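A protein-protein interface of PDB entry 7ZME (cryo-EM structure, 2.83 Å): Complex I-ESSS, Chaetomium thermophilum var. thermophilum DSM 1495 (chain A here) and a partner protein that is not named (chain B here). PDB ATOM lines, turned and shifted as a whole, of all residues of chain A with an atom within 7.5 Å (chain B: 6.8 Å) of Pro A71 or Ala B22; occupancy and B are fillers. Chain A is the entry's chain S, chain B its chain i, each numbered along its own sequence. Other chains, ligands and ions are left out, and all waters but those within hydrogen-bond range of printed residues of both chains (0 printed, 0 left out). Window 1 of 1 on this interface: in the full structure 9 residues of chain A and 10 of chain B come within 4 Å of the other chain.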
ATOM      1  N   TYR A  68     -24.147  -2.423 -20.860  1.00  0.00           N
ATOM      2  CA  TYR A  68     -24.993  -3.591 -21.034  1.00  0.00           C
ATOM      3  C   TYR A  68     -24.380  -4.515 -22.073  1.00  0.00           C
ATOM      4  O   TYR A  68     -23.636  -4.079 -22.955  1.00  0.00           O
ATOM      5  CB  TYR A  68     -26.411  -3.209 -21.460  1.00  0.00           C
ATOM      6  CG  TYR A  68     -27.182  -2.449 -20.413  1.00  0.00           C
ATOM      7  CD1 TYR A  68     -27.775  -3.107 -19.348  1.00  0.00           C
ATOM      8  CD2 TYR A  68     -27.355  -1.078 -20.512  1.00  0.00           C
ATOM      9  CE1 TYR A  68     -28.487  -2.416 -18.391  1.00  0.00           C
ATOM     10  CE2 TYR A  68     -28.071  -0.379 -19.564  1.00  0.00           C
ATOM     11  CZ  TYR A  68     -28.636  -1.054 -18.506  1.00  0.00           C
ATOM     12  OH  TYR A  68     -29.350  -0.363 -17.557  1.00  0.00           O
ATOM     13  N   ASP A  69     -24.695  -5.774 -21.963  1.00  0.00           N
ATOM     14  CA  ASP A  69     -24.170  -6.776 -22.870  1.00  0.00           C
ATOM     15  C   ASP A  69     -25.168  -7.076 -23.982  1.00  0.00           C
ATOM     16  O   ASP A  69     -26.381  -6.976 -23.780  1.00  0.00           O
ATOM     17  CB  ASP A  69     -23.852  -8.068 -22.114  1.00  0.00           C
ATOM     18  CG  ASP A  69     -22.984  -7.833 -20.894  1.00  0.00           C
ATOM     19  OD1 ASP A  69     -22.487  -6.701 -20.724  1.00  0.00           O
ATOM     20  OD2 ASP A  69     -22.792  -8.783 -20.107  1.00  0.00           O
ATOM     21  N   PRO A  70     -24.700  -7.429 -25.180  1.00  0.00           N
ATOM     22  CA  PRO A  70     -25.630  -7.851 -26.222  1.00  0.00           C
ATOM     23  C   PRO A  70     -26.268  -9.179 -25.861  1.00  0.00           C
ATOM     24  O   PRO A  70     -25.649 -10.016 -25.183  1.00  0.00           O
ATOM     25  CB  PRO A  70     -24.731  -7.977 -27.465  1.00  0.00           C
ATOM     26  CG  PRO A  70     -23.381  -8.266 -26.910  1.00  0.00           C
ATOM     27  CD  PRO A  70     -23.298  -7.487 -25.627  1.00  0.00           C
ATOM     28  N   PRO A  71     -27.510  -9.414 -26.278  1.00  0.00           N
ATOM     29  CA  PRO A  71     -28.146 -10.704 -25.995  1.00  0.00           C
ATOM     30  C   PRO A  71     -27.383 -11.844 -26.649  1.00  0.00           C
ATOM     31  O   PRO A  71     -26.845 -11.708 -27.750  1.00  0.00           O
ATOM     32  CB  PRO A  71     -29.548 -10.545 -26.591  1.00  0.00           C
ATOM     33  CG  PRO A  71     -29.778  -9.077 -26.580  1.00  0.00           C
ATOM     34  CD  PRO A  71     -28.442  -8.490 -26.935  1.00  0.00           C
ATOM     35  N   THR A  72     -27.337 -12.977 -25.956  1.00  0.00           N
ATOM     36  CA  THR A  72     -26.551 -14.107 -26.416  1.00  0.00           C
ATOM     37  C   THR A  72     -27.249 -15.394 -26.010  1.00  0.00           C
ATOM     38  O   THR A  72     -28.211 -15.392 -25.239  1.00  0.00           O
ATOM     39  CB  THR A  72     -25.125 -14.061 -25.855  1.00  0.00           C
ATOM     40  OG1 THR A  72     -24.320 -15.051 -26.505  1.00  0.00           O
ATOM     41  CG2 THR A  72     -25.136 -14.323 -24.358  1.00  0.00           C
ATOM     42  N   GLY A  73     -26.747 -16.501 -26.544  1.00  0.00           N
ATOM     43  CA  GLY A  73     -27.304 -17.801 -26.259  1.00  0.00           C
ATOM     44  C   GLY A  73     -27.534 -18.597 -27.521  1.00  0.00           C
ATOM     45  O   GLY A  73     -27.592 -18.032 -28.616  1.00  0.00           O
ATOM     46  N   TYR B   9     -21.127 -15.086 -16.700  1.00  0.00           N
ATOM     47  CA  TYR B   9     -22.275 -15.921 -17.017  1.00  0.00           C
ATOM     48  C   TYR B   9     -21.989 -16.669 -18.308  1.00  0.00           C
ATOM     49  O   TYR B   9     -21.128 -16.251 -19.091  1.00  0.00           O
ATOM     50  CB  TYR B   9     -23.549 -15.078 -17.153  1.00  0.00           C
ATOM     51  CG  TYR B   9     -23.442 -13.980 -18.175  1.00  0.00           C
ATOM     52  CD1 TYR B   9     -22.942 -12.736 -17.832  1.00  0.00           C
ATOM     53  CD2 TYR B   9     -23.851 -14.185 -19.482  1.00  0.00           C
ATOM     54  CE1 TYR B   9     -22.845 -11.733 -18.760  1.00  0.00           C
ATOM     55  CE2 TYR B   9     -23.761 -13.187 -20.414  1.00  0.00           C
ATOM     56  CZ  TYR B   9     -23.257 -11.962 -20.050  1.00  0.00           C
ATOM     57  OH  TYR B   9     -23.162 -10.959 -20.981  1.00  0.00           O
ATOM     58  N   SER B  15     -32.186 -16.963 -23.258  1.00  0.00           N
ATOM     59  CA  SER B  15     -33.312 -16.610 -22.420  1.00  0.00           C
ATOM     60  C   SER B  15     -34.289 -15.736 -23.194  1.00  0.00           C
ATOM     61  O   SER B  15     -33.867 -14.896 -23.993  1.00  0.00           O
ATOM     62  CB  SER B  15     -32.843 -15.865 -21.163  1.00  0.00           C
ATOM     63  OG  SER B  15     -33.935 -15.488 -20.349  1.00  0.00           O
ATOM     64  N   ALA B  17     -36.415 -13.586 -21.666  1.00  0.00           N
ATOM     65  CA  ALA B  17     -36.314 -12.313 -20.967  1.00  0.00           C
ATOM     66  C   ALA B  17     -34.971 -11.632 -21.186  1.00  0.00           C
ATOM     67  O   ALA B  17     -34.743 -10.556 -20.630  1.00  0.00           O
ATOM     68  CB  ALA B  17     -36.568 -12.515 -19.474  1.00  0.00           C
ATOM     69  N   GLY B  18     -34.081 -12.230 -21.969  1.00  0.00           N
ATOM     70  CA  GLY B  18     -32.868 -11.559 -22.379  1.00  0.00           C
ATOM     71  C   GLY B  18     -31.580 -12.213 -21.937  1.00  0.00           C
ATOM     72  O   GLY B  18     -30.649 -12.356 -22.735  1.00  0.00           O
ATOM     73  N   GLY B  19     -31.511 -12.640 -20.684  1.00  0.00           N
ATOM     74  CA  GLY B  19     -30.274 -13.199 -20.185  1.00  0.00           C
ATOM     75  C   GLY B  19     -29.734 -12.447 -18.992  1.00  0.00           C
ATOM     76  O   GLY B  19     -30.452 -12.235 -18.015  1.00  0.00           O
ATOM     77  N   TRP B  20     -28.467 -12.036 -19.047  1.00  0.00           N
ATOM     78  CA  TRP B  20     -27.834 -11.417 -17.890  1.00  0.00           C
ATOM     79  C   TRP B  20     -27.785  -9.897 -17.975  1.00  0.00           C
ATOM     80  O   TRP B  20     -28.340  -9.220 -17.114  1.00  0.00           O
ATOM     81  CB  TRP B  20     -26.439 -12.005 -17.673  1.00  0.00           C
ATOM     82  CG  TRP B  20     -26.489 -13.217 -16.815  1.00  0.00           C
ATOM     83  CD1 TRP B  20     -26.253 -13.276 -15.476  1.00  0.00           C
ATOM     84  CD2 TRP B  20     -26.845 -14.540 -17.220  1.00  0.00           C
ATOM     85  NE1 TRP B  20     -26.412 -14.559 -15.023  1.00  0.00           N
ATOM     86  CE2 TRP B  20     -26.778 -15.356 -16.076  1.00  0.00           C
ATOM     87  CE3 TRP B  20     -27.192 -15.119 -18.441  1.00  0.00           C
ATOM     88  CZ2 TRP B  20     -27.047 -16.715 -16.117  1.00  0.00           C
ATOM     89  CZ3 TRP B  20     -27.462 -16.466 -18.480  1.00  0.00           C
ATOM     90  CH2 TRP B  20     -27.386 -17.251 -17.326  1.00  0.00           C
ATOM     91  N   TYR B  21     -27.154  -9.338 -18.992  1.00  0.00           N
ATOM     92  CA  TYR B  21     -27.159  -7.887 -19.122  1.00  0.00           C
ATOM     93  C   TYR B  21     -27.597  -7.500 -20.515  1.00  0.00           C
ATOM     94  O   TYR B  21     -27.028  -6.609 -21.149  1.00  0.00           O
ATOM     95  CB  TYR B  21     -25.793  -7.299 -18.777  1.00  0.00           C
ATOM     96  CG  TYR B  21     -25.404  -7.502 -17.329  1.00  0.00           C
ATOM     97  CD1 TYR B  21     -24.810  -8.683 -16.909  1.00  0.00           C
ATOM     98  CD2 TYR B  21     -25.643  -6.519 -16.381  1.00  0.00           C
ATOM     99  CE1 TYR B  21     -24.463  -8.876 -15.590  1.00  0.00           C
ATOM    100  CE2 TYR B  21     -25.297  -6.702 -15.061  1.00  0.00           C
ATOM    101  CZ  TYR B  21     -24.707  -7.882 -14.671  1.00  0.00           C
ATOM    102  OH  TYR B  21     -24.360  -8.067 -13.354  1.00  0.00           O
ATOM    103  N   ALA B  22     -28.649  -8.157 -20.995  1.00  0.00           N
ATOM    104  CA  ALA B  22     -28.978  -8.176 -22.412  1.00  0.00           C
ATOM    105  C   ALA B  22     -29.611  -6.858 -22.835  1.00  0.00           C
ATOM    106  O   ALA B  22     -30.709  -6.512 -22.389  1.00  0.00           O
ATOM    107  CB  ALA B  22     -29.905  -9.346 -22.716  1.00  0.00           C
ATOM    108  N   GLN B  23     -28.888  -6.103 -23.652  1.00  0.00           N
ATOM    109  CA  GLN B  23     -29.480  -4.922 -24.295  1.00  0.00           C
ATOM    110  C   GLN B  23     -29.075  -5.096 -25.749  1.00  0.00           C
ATOM    111  O   GLN B  23     -27.878  -5.178 -26.019  1.00  0.00           O
ATOM    112  CB  GLN B  23     -29.023  -3.598 -23.704  1.00  0.00           C
ATOM    113  CG  GLN B  23     -29.656  -2.400 -24.397  1.00  0.00           C
ATOM    114  CD  GLN B  23     -30.043  -1.293 -23.451  1.00  0.00           C
ATOM    115  OE1 GLN B  23     -30.877  -1.462 -22.573  1.00  0.00           O
ATOM    116  NE2 GLN B  23     -29.440  -0.132 -23.638  1.00  0.00           N
ATOM    117  N   PRO B  24     -30.023  -5.211 -26.684  1.00  0.00           N
ATOM    118  CA  PRO B  24     -29.685  -5.323 -28.073  1.00  0.00           C
ATOM    119  C   PRO B  24     -29.163  -3.988 -28.627  1.00  0.00           C
ATOM    120  O   PRO B  24     -29.334  -2.972 -27.992  1.00  0.00           O
ATOM    121  CB  PRO B  24     -31.007  -5.822 -28.660  1.00  0.00           C
ATOM    122  CG  PRO B  24     -32.038  -5.179 -27.816  1.00  0.00           C
ATOM    123  CD  PRO B  24     -31.446  -5.297 -26.436  1.00  0.00           C
ATOM    124  N   ALA B  25     -28.457  -4.030 -29.750  1.00  0.00           N
ATOM    125  CA  ALA B  25     -27.972  -2.790 -30.406  1.00  0.00           C
ATOM    126  C   ALA B  25     -29.152  -2.033 -31.012  1.00  0.00           C
ATOM    127  O   ALA B  25     -29.019  -0.826 -31.246  1.00  0.00           O
ATOM    128  CB  ALA B  25     -26.946  -3.127 -31.454  1.00  0.00           C
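Pro A71 touches three residues of chain B. Printed residues of chain B within 4 Å of Pro A70: Gln B23 (3.5 Å). Of the printed residues of chain B, Asp A69 touches Tyr B9 (2.4 Å), Tyr B21 (2.6 Å), Ala B22 (3.2 Å) and Gln B23 (2.7 Å). Printed residues of chain A within 4 Å of Tyr B9: Asp A69. Printed residues of chain A within 4 Å of Pro B24: Pro A71. The nearest printed residue of chain B that does not touch Pro A70 is Ala B22 (4.5 Å).
The backbone NH of Asp A69 lies within hydrogen-bond range of the backbone carbonyl oxygen of Tyr B21, 2.6 Å away. The backbone carbonyl oxygen (O) of Asp A69 is in hydrogen-bond range of the backbone NH (N) of Gln B23, at 2.7 Å. OD2 of Asp A69 sits close to OH of Tyr B9 (2.4 Å).
O of Tyr B21 touches CB of Tyr A68 (3.5 Å). Gln B23 touches Tyr A68. Asp A69 touches Ala B22. CA of Pro A70 touches O of Gln B23 (3.5 Å). Pro A71 touches Ala B22. Gln B23 touches Pro A71. Pro A71 touches Pro B24 (CD to CA, 3.6 Å).
Printed residues of chain A that touch a printed residue of chain B: Tyr A68, Asp A69, Pro A70 and Pro A71. Hydrophobic or aromatic side chains of chain A within 4 Å of the printed part of chain B: Tyr A68 and Pro A71. Hydrophobic or aromatic side chains of chain B that line the printed part of chain A: Tyr B9, Tyr B21 and Ala B22. Among the printed residues, 10 pairs touch across the chains.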
